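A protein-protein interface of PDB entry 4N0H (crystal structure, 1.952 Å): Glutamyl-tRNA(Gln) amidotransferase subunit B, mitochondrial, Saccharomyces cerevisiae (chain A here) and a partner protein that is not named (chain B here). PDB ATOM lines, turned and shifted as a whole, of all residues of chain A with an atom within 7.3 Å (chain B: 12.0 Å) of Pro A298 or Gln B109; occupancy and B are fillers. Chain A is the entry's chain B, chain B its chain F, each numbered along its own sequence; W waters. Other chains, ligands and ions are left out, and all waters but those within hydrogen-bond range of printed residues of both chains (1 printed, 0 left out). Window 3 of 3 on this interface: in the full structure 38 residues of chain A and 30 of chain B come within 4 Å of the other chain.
ND2 of Asn A295 sits close to O of Thr B107 (3.4 Å).
OD1 of Asn A295 lies within hydrogen-bond range of NE2 of Gln B109 (3.3 Å).
The backbone NH (N) of Leu B110 lies within hydrogen-bond range of the backbone carbonyl oxygen (O) of Asn A295 (2.8 Å).
The side-chain amide nitrogen (NE2) of Gln B109 sits at hydrogen-bond distance from the backbone carbonyl oxygen (O) of Leu A296 (3.4 Å).
The backbone NH (N) of Ala A297 sits at hydrogen-bond distance from the backbone carbonyl oxygen (O) of Leu B110.
The side-chain carboxylate (OD2) of Asp A299 sits at hydrogen-bond distance from the backbone NH (N) of Tyr B112 (3.0 Å).
O of Gly A303 is in hydrogen-bond range of OH of Tyr B112 (3.5 Å).
O of Ser A84 sits close to OD1 of Asn A295 (3.4 Å).
The side-chain hydroxyl (OG) of Ser A302 sits at hydrogen-bond distance from the backbone carbonyl oxygen (O) of Asp A299 (3.4 Å).
ND2 of Asn B111 lies within hydrogen-bond range of OG1 of Thr B113, 3.4 Å away.
The side-chain amide nitrogen of Asn B111 sits close to the backbone NH of Lys B114.
Among the printed residues, merely in contact across the chains: Val A300 with Leu B110 (3.3 Å), Asp A299 with Asn B111 (3.3 Å), Leu A296 with Leu B110 (3.5 Å), Ala A297 with Gln B109 (3.6 Å), Val A300 with Asn B111 (3.6 Å), Val A300 with Tyr B112 (3.7 Å), Pro A298 with Gln B109 (3.7 Å) and Ala A297 with Asn B111 (3.9 Å).
Of chain B, only Thr B107 (3.3 Å), Gln B109 (3.2 Å) and Leu B110 (2.8 Å) come within 4 Å of Asn A295.
Printed residues of chain B within 4 Å of Leu A296: Gln B109 (3.4 Å) and Leu B110 (3.5 Å).
Of chain B, only Asn B111 and Tyr B112 come within 4 Å of Asp A299.
Of chain B, only Leu B110 (3.3 Å), Asn B111 (3.6 Å) and Tyr B112 (3.7 Å) come within 4 Å of Val A300.
No residue of chain B comes within 4 Å of Ile A301.
No residue of chain B comes within 4 Å of Ser A302.
Printed residues of chain B within 4 Å of Gly A303: Tyr B112.
Gln B109 touches just these residues of chain A: Asn A295 (3.2 Å), Leu A296 (3.4 Å), Ala A297 (3.6 Å) and Pro A298 (3.7 Å).
Of the printed residues of chain A, Leu B110 touches Asn A295, Leu A296, Ala A297 and Val A300.
Of the printed residues of chain A, Tyr B112 touches Asp A299 (3.0 Å), Val A300 (3.7 Å) and Gly A303 (3.4 Å).
The nearest printed residue of chain B that does not touch Leu A296 is Leu B115 (5.5 Å).
Printed residues of chain A that touch a printed residue of chain B: Asn A295, Leu A296, Ala A297, Pro A298, Asp A299, Val A300 and Gly A303.
Hydrophobic or aromatic side chains of chain A that line the printed part of chain B: Leu A296, Ala A297, Pro A298 and Val A300.
Hydrophobic or aromatic side chains of chain B that line the printed part of chain A: Leu B110 and Tyr B112.
Among the printed residues, no Asp or Glu carboxylate lies within 4 Å of a Lys or Arg side-chain nitrogen of the other chain.
Water W1 lies within hydrogen-bond range of OD1 of Asp A299 and N of Thr B113.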
ATOM      1  N   MET A  72     -19.759 -24.197 -11.503  1.00  0.00           N
ATOM      2  CA  MET A  72     -18.562 -23.432 -11.150  1.00  0.00           C
ATOM      3  C   MET A  72     -18.118 -22.523 -12.296  1.00  0.00           C
ATOM      4  O   MET A  72     -17.857 -21.337 -12.094  1.00  0.00           O
ATOM      5  CB  MET A  72     -17.417 -24.370 -10.762  1.00  0.00           C
ATOM      6  CG  MET A  72     -17.265 -24.562  -9.264  1.00  0.00           C
ATOM      7  SD  MET A  72     -16.915 -22.985  -8.460  1.00  0.00           S
ATOM      8  CE  MET A  72     -16.582 -23.536  -6.799  1.00  0.00           C
ATOM      9  N   SER A  84     -20.721 -20.887   0.355  1.00  0.00           N
ATOM     10  CA  SER A  84     -19.851 -21.758   1.140  1.00  0.00           C
ATOM     11  C   SER A  84     -20.510 -23.115   1.338  1.00  0.00           C
ATOM     12  O   SER A  84     -19.864 -24.158   1.237  1.00  0.00           O
ATOM     13  CB  SER A  84     -19.540 -21.122   2.494  1.00  0.00           C
ATOM     14  OG  SER A  84     -20.735 -20.807   3.185  1.00  0.00           O
ATOM     15  N   ILE A  85     -21.809 -23.086   1.612  1.00  0.00           N
ATOM     16  CA  ILE A  85     -22.615 -24.292   1.698  1.00  0.00           C
ATOM     17  C   ILE A  85     -23.853 -24.116   0.832  1.00  0.00           C
ATOM     18  O   ILE A  85     -24.597 -23.150   0.998  1.00  0.00           O
ATOM     19  CB  ILE A  85     -23.095 -24.548   3.139  1.00  0.00           C
ATOM     20  CG1 ILE A  85     -21.910 -24.802   4.074  1.00  0.00           C
ATOM     21  CG2 ILE A  85     -24.069 -25.718   3.182  1.00  0.00           C
ATOM     22  CD1 ILE A  85     -21.252 -26.144   3.870  1.00  0.00           C
ATOM     23  N   ILE A 294     -23.403 -29.246  -0.375  1.00  0.00           N
ATOM     24  CA  ILE A 294     -22.306 -28.931  -1.275  1.00  0.00           C
ATOM     25  C   ILE A 294     -21.351 -28.018  -0.513  1.00  0.00           C
ATOM     26  O   ILE A 294     -21.686 -26.872  -0.228  1.00  0.00           O
ATOM     27  CB  ILE A 294     -22.803 -28.219  -2.552  1.00  0.00           C
ATOM     28  CG1 ILE A 294     -23.644 -29.172  -3.402  1.00  0.00           C
ATOM     29  CG2 ILE A 294     -21.631 -27.668  -3.373  1.00  0.00           C
ATOM     30  CD1 ILE A 294     -24.179 -28.543  -4.668  1.00  0.00           C
ATOM     31  N   ASN A 295     -20.177 -28.537  -0.169  1.00  0.00           N
ATOM     32  CA  ASN A 295     -19.183 -27.776   0.586  1.00  0.00           C
ATOM     33  C   ASN A 295     -17.838 -27.780  -0.126  1.00  0.00           C
ATOM     34  O   ASN A 295     -17.020 -28.670   0.082  1.00  0.00           O
ATOM     35  CB  ASN A 295     -19.034 -28.352   1.995  1.00  0.00           C
ATOM     36  CG  ASN A 295     -18.096 -27.537   2.867  1.00  0.00           C
ATOM     37  OD1 ASN A 295     -17.691 -26.430   2.509  1.00  0.00           O
ATOM     38  ND2 ASN A 295     -17.750 -28.084   4.024  1.00  0.00           N
ATOM     39  N   LEU A 296     -17.616 -26.780  -0.973  1.00  0.00           N
ATOM     40  CA  LEU A 296     -16.436 -26.759  -1.826  1.00  0.00           C
ATOM     41  C   LEU A 296     -15.257 -26.095  -1.126  1.00  0.00           C
ATOM     42  O   LEU A 296     -15.415 -25.079  -0.452  1.00  0.00           O
ATOM     43  CB  LEU A 296     -16.760 -26.039  -3.137  1.00  0.00           C
ATOM     44  CG  LEU A 296     -17.991 -26.642  -3.825  1.00  0.00           C
ATOM     45  CD1 LEU A 296     -18.460 -25.777  -4.979  1.00  0.00           C
ATOM     46  CD2 LEU A 296     -17.689 -28.052  -4.295  1.00  0.00           C
ATOM     47  N   ALA A 297     -14.078 -26.689  -1.276  1.00  0.00           N
ATOM     48  CA  ALA A 297     -12.862 -26.110  -0.721  1.00  0.00           C
ATOM     49  C   ALA A 297     -12.436 -24.953  -1.607  1.00  0.00           C
ATOM     50  O   ALA A 297     -12.750 -24.937  -2.798  1.00  0.00           O
ATOM     51  CB  ALA A 297     -11.758 -27.152  -0.641  1.00  0.00           C
ATOM     52  N   PRO A 298     -11.734 -23.967  -1.025  1.00  0.00           N
ATOM     53  CA  PRO A 298     -11.256 -22.804  -1.777  1.00  0.00           C
ATOM     54  C   PRO A 298     -10.493 -23.158  -3.062  1.00  0.00           C
ATOM     55  O   PRO A 298     -10.551 -22.385  -4.016  1.00  0.00           O
ATOM     56  CB  PRO A 298     -10.324 -22.090  -0.782  1.00  0.00           C
ATOM     57  CG  PRO A 298     -10.392 -22.878   0.512  1.00  0.00           C
ATOM     58  CD  PRO A 298     -11.577 -23.779   0.427  1.00  0.00           C
ATOM     59  N   ASP A 299      -9.811 -24.302  -3.096  1.00  0.00           N
ATOM     60  CA  ASP A 299      -9.000 -24.653  -4.263  1.00  0.00           C
ATOM     61  C   ASP A 299      -9.829 -25.105  -5.468  1.00  0.00           C
ATOM     62  O   ASP A 299      -9.292 -25.299  -6.559  1.00  0.00           O
ATOM     63  CB  ASP A 299      -7.917 -25.690  -3.919  1.00  0.00           C
ATOM     64  CG  ASP A 299      -8.485 -27.066  -3.579  1.00  0.00           C
ATOM     65  OD1 ASP A 299      -7.692 -27.931  -3.147  1.00  0.00           O
ATOM     66  OD2 ASP A 299      -9.703 -27.300  -3.737  1.00  0.00           O
ATOM     67  N   VAL A 300     -11.128 -25.299  -5.258  1.00  0.00           N
ATOM     68  CA  VAL A 300     -12.023 -25.600  -6.370  1.00  0.00           C
ATOM     69  C   VAL A 300     -12.168 -24.340  -7.223  1.00  0.00           C
ATOM     70  O   VAL A 300     -12.191 -24.408  -8.451  1.00  0.00           O
ATOM     71  CB  VAL A 300     -13.407 -26.092  -5.889  1.00  0.00           C
ATOM     72  CG1 VAL A 300     -14.328 -26.352  -7.075  1.00  0.00           C
ATOM     73  CG2 VAL A 300     -13.265 -27.355  -5.058  1.00  0.00           C
ATOM     74  N   ILE A 301     -12.240 -23.190  -6.555  1.00  0.00           N
ATOM     75  CA  ILE A 301     -12.325 -21.898  -7.232  1.00  0.00           C
ATOM     76  C   ILE A 301     -11.119 -21.637  -8.129  1.00  0.00           C
ATOM     77  O   ILE A 301     -11.267 -21.376  -9.322  1.00  0.00           O
ATOM     78  CB  ILE A 301     -12.423 -20.743  -6.230  1.00  0.00           C
ATOM     79  CG1 ILE A 301     -13.549 -20.992  -5.227  1.00  0.00           C
ATOM     80  CG2 ILE A 301     -12.631 -19.431  -6.968  1.00  0.00           C
ATOM     81  CD1 ILE A 301     -14.923 -20.678  -5.766  1.00  0.00           C
ATOM     82  N   SER A 302      -9.921 -21.705  -7.554  1.00  0.00           N
ATOM     83  CA  SER A 302      -8.703 -21.487  -8.332  1.00  0.00           C
ATOM     84  C   SER A 302      -8.485 -22.586  -9.373  1.00  0.00           C
ATOM     85  O   SER A 302      -8.011 -22.316 -10.470  1.00  0.00           O
ATOM     86  CB  SER A 302      -7.479 -21.358  -7.418  1.00  0.00           C
ATOM     87  OG  SER A 302      -7.483 -22.370  -6.423  1.00  0.00           O
ATOM     88  N   GLY A 303      -8.840 -23.819  -9.027  1.00  0.00           N
ATOM     89  CA  GLY A 303      -8.689 -24.938  -9.942  1.00  0.00           C
ATOM     90  C   GLY A 303      -9.501 -24.780 -11.216  1.00  0.00           C
ATOM     91  O   GLY A 303      -8.966 -24.867 -12.324  1.00  0.00           O
ATOM     92  N   ARG A 305     -10.838 -22.084 -12.281  1.00  0.00           N
ATOM     93  CA  ARG A 305     -10.430 -20.837 -12.928  1.00  0.00           C
ATOM     94  C   ARG A 305      -9.408 -21.090 -14.031  1.00  0.00           C
ATOM     95  O   ARG A 305      -9.460 -20.473 -15.096  1.00  0.00           O
ATOM     96  CB  ARG A 305      -9.853 -19.856 -11.903  1.00  0.00           C
ATOM     97  CG  ARG A 305     -10.605 -18.538 -11.819  1.00  0.00           C
ATOM     98  CD  ARG A 305     -10.068 -17.644 -10.709  1.00  0.00           C
ATOM     99  NE  ARG A 305     -11.024 -16.594 -10.364  1.00  0.00           N
ATOM    100  CZ  ARG A 305     -11.355 -16.265  -9.121  1.00  0.00           C
ATOM    101  NH1 ARG A 305     -10.799 -16.896  -8.098  1.00  0.00           N
ATOM    102  NH2 ARG A 305     -12.240 -15.304  -8.896  1.00  0.00           N
ATOM    103  N   ASN B 106     -17.606 -26.590   9.363  1.00  0.00           N
ATOM    104  CA  ASN B 106     -16.389 -27.333   9.665  1.00  0.00           C
ATOM    105  C   ASN B 106     -16.511 -28.816   9.324  1.00  0.00           C
ATOM    106  O   ASN B 106     -16.107 -29.677  10.108  1.00  0.00           O
ATOM    107  CB  ASN B 106     -16.002 -27.159  11.135  1.00  0.00           C
ATOM    108  N   THR B 107     -17.069 -29.108   8.154  1.00  0.00           N
ATOM    109  CA  THR B 107     -17.199 -30.491   7.702  1.00  0.00           C
ATOM    110  C   THR B 107     -16.330 -30.775   6.478  1.00  0.00           C
ATOM    111  O   THR B 107     -15.596 -29.905   6.005  1.00  0.00           O
ATOM    112  CB  THR B 107     -18.666 -30.867   7.402  1.00  0.00           C
ATOM    113  OG1 THR B 107     -18.739 -32.249   7.031  1.00  0.00           O
ATOM    114  CG2 THR B 107     -19.226 -30.009   6.276  1.00  0.00           C
ATOM    115  N   LYS B 108     -16.427 -32.000   5.971  1.00  0.00           N
ATOM    116  CA  LYS B 108     -15.575 -32.476   4.884  1.00  0.00           C
ATOM    117  C   LYS B 108     -15.803 -31.716   3.572  1.00  0.00           C
ATOM    118  O   LYS B 108     -16.826 -31.893   2.906  1.00  0.00           O
ATOM    119  CB  LYS B 108     -15.794 -33.976   4.673  1.00  0.00           C
ATOM    120  CG  LYS B 108     -14.693 -34.676   3.899  1.00  0.00           C
ATOM    121  CD  LYS B 108     -15.200 -35.208   2.569  1.00  0.00           C
ATOM    122  CE  LYS B 108     -14.258 -36.258   2.010  1.00  0.00           C
ATOM    123  NZ  LYS B 108     -12.844 -35.789   2.002  1.00  0.00           N
ATOM    124  N   GLN B 109     -14.840 -30.873   3.209  1.00  0.00           N
ATOM    125  CA  GLN B 109     -14.926 -30.110   1.971  1.00  0.00           C
ATOM    126  C   GLN B 109     -14.502 -30.935   0.761  1.00  0.00           C
ATOM    127  O   GLN B 109     -13.512 -31.667   0.813  1.00  0.00           O
ATOM    128  CB  GLN B 109     -14.068 -28.841   2.049  1.00  0.00           C
ATOM    129  CG  GLN B 109     -14.625 -27.755   2.954  1.00  0.00           C
ATOM    130  CD  GLN B 109     -13.835 -26.460   2.867  1.00  0.00           C
ATOM    131  OE1 GLN B 109     -12.602 -26.471   2.818  1.00  0.00           O
ATOM    132  NE2 GLN B 109     -14.544 -25.337   2.839  1.00  0.00           N
ATOM    133  N   LEU B 110     -15.255 -30.812  -0.329  1.00  0.00           N
ATOM    134  CA  LEU B 110     -14.848 -31.381  -1.609  1.00  0.00           C
ATOM    135  C   LEU B 110     -13.814 -30.462  -2.250  1.00  0.00           C
ATOM    136  O   LEU B 110     -14.122 -29.314  -2.567  1.00  0.00           O
ATOM    137  CB  LEU B 110     -16.055 -31.526  -2.542  1.00  0.00           C
ATOM    138  CG  LEU B 110     -15.772 -32.078  -3.942  1.00  0.00           C
ATOM    139  CD1 LEU B 110     -15.520 -33.575  -3.895  1.00  0.00           C
ATOM    140  CD2 LEU B 110     -16.926 -31.766  -4.873  1.00  0.00           C
ATOM    141  N   ASN B 111     -12.591 -30.953  -2.430  1.00  0.00           N
ATOM    142  CA  ASN B 111     -11.559 -30.150  -3.073  1.00  0.00           C
ATOM    143  C   ASN B 111     -11.429 -30.437  -4.564  1.00  0.00           C
ATOM    144  O   ASN B 111     -12.142 -31.283  -5.107  1.00  0.00           O
ATOM    145  CB  ASN B 111     -10.200 -30.246  -2.354  1.00  0.00           C
ATOM    146  CG  ASN B 111      -9.660 -31.669  -2.266  1.00  0.00           C
ATOM    147  OD1 ASN B 111      -9.202 -32.093  -1.206  1.00  0.00           O
ATOM    148  ND2 ASN B 111      -9.693 -32.402  -3.375  1.00  0.00           N
ATOM    149  N   TYR B 112     -10.501 -29.743  -5.212  1.00  0.00           N
ATOM    150  CA  TYR B 112     -10.393 -29.774  -6.663  1.00  0.00           C
ATOM    151  C   TYR B 112     -10.063 -31.152  -7.241  1.00  0.00           C
ATOM    152  O   TYR B 112     -10.742 -31.612  -8.158  1.00  0.00           O
ATOM    153  CB  TYR B 112      -9.390 -28.728  -7.157  1.00  0.00           C
ATOM    154  CG  TYR B 112      -9.340 -28.612  -8.663  1.00  0.00           C
ATOM    155  CD1 TYR B 112      -8.201 -28.971  -9.370  1.00  0.00           C
ATOM    156  CD2 TYR B 112     -10.441 -28.158  -9.380  1.00  0.00           C
ATOM    157  CE1 TYR B 112      -8.155 -28.870 -10.747  1.00  0.00           C
ATOM    158  CE2 TYR B 112     -10.407 -28.059 -10.758  1.00  0.00           C
ATOM    159  CZ  TYR B 112      -9.261 -28.413 -11.434  1.00  0.00           C
ATOM    160  OH  TYR B 112      -9.217 -28.315 -12.804  1.00  0.00           O
ATOM    161  N   THR B 113      -9.027 -31.807  -6.720  1.00  0.00           N
ATOM    162  CA  THR B 113      -8.640 -33.111  -7.252  1.00  0.00           C
ATOM    163  C   THR B 113      -9.738 -34.149  -7.034  1.00  0.00           C
ATOM    164  O   THR B 113      -9.994 -34.975  -7.904  1.00  0.00           O
ATOM    165  CB  THR B 113      -7.307 -33.631  -6.665  1.00  0.00           C
ATOM    166  OG1 THR B 113      -7.511 -34.092  -5.326  1.00  0.00           O
ATOM    167  CG2 THR B 113      -6.245 -32.542  -6.682  1.00  0.00           C
ATOM    168  N   LYS B 114     -10.389 -34.094  -5.876  1.00  0.00           N
ATOM    169  CA  LYS B 114     -11.503 -34.991  -5.584  1.00  0.00           C
ATOM    170  C   LYS B 114     -12.693 -34.722  -6.497  1.00  0.00           C
ATOM    171  O   LYS B 114     -13.387 -35.654  -6.908  1.00  0.00           O
ATOM    172  CB  LYS B 114     -11.924 -34.882  -4.118  1.00  0.00           C
ATOM    173  CG  LYS B 114     -10.882 -35.413  -3.153  1.00  0.00           C
ATOM    174  CD  LYS B 114     -10.398 -36.784  -3.591  1.00  0.00           C
ATOM    175  CE  LYS B 114      -9.204 -37.237  -2.770  1.00  0.00           C
ATOM    176  NZ  LYS B 114      -8.781 -38.617  -3.137  1.00  0.00           N
ATOM    177  N   LEU B 115     -12.924 -33.447  -6.807  1.00  0.00           N
ATOM    178  CA  LEU B 115     -13.948 -33.054  -7.768  1.00  0.00           C
ATOM    179  C   LEU B 115     -13.688 -33.747  -9.100  1.00  0.00           C
ATOM    180  O   LEU B 115     -14.571 -34.401  -9.653  1.00  0.00           O
ATOM    181  CB  LEU B 115     -13.935 -31.536  -7.971  1.00  0.00           C
ATOM    182  CG  LEU B 115     -15.198 -30.785  -8.417  1.00  0.00           C
ATOM    183  CD1 LEU B 115     -14.861 -29.702  -9.440  1.00  0.00           C
ATOM    184  CD2 LEU B 115     -16.304 -31.698  -8.930  1.00  0.00           C
ATOM    185  N   LEU B 116     -12.465 -33.605  -9.602  1.00  0.00           N
ATOM    186  CA  LEU B 116     -12.085 -34.148 -10.901  1.00  0.00           C
ATOM    187  C   LEU B 116     -11.933 -35.669 -10.892  1.00  0.00           C
ATOM    188  O   LEU B 116     -12.201 -36.327 -11.897  1.00  0.00           O
ATOM    189  CB  LEU B 116     -10.793 -33.492 -11.394  1.00  0.00           C
ATOM    190  CG  LEU B 116     -10.947 -32.303 -12.348  1.00  0.00           C
ATOM    191  CD1 LEU B 116     -11.981 -31.318 -11.849  1.00  0.00           C
ATOM    192  CD2 LEU B 116      -9.610 -31.615 -12.556  1.00  0.00           C
ATOM    193  N   GLU B 117     -11.491 -36.224  -9.767  1.00  0.00           N
ATOM    194  CA  GLU B 117     -11.372 -37.673  -9.644  1.00  0.00           C
ATOM    195  C   GLU B 117     -12.752 -38.313  -9.554  1.00  0.00           C
ATOM    196  O   GLU B 117     -13.002 -39.361 -10.148  1.00  0.00           O
ATOM    197  CB  GLU B 117     -10.537 -38.055  -8.422  1.00  0.00           C
ATOM    198  CG  GLU B 117     -10.375 -39.555  -8.236  1.00  0.00           C
ATOM    199  CD  GLU B 117      -9.346 -39.904  -7.176  1.00  0.00           C
ATOM    200  OE1 GLU B 117      -9.502 -39.456  -6.020  1.00  0.00           O
ATOM    201  OE2 GLU B 117      -8.376 -40.621  -7.506  1.00  0.00           O
ATOM    202  N   GLY B 118     -13.644 -37.673  -8.805  1.00  0.00           N
ATOM    203  CA  GLY B 118     -15.012 -38.141  -8.679  1.00  0.00           C
ATOM    204  C   GLY B 118     -15.691 -38.195 -10.034  1.00  0.00           C
ATOM    205  O   GLY B 118     -16.322 -39.193 -10.375  1.00  0.00           O
HETATM  206  O   HOH W   1      -7.085 -30.270  -4.535  1.00  0.00           O
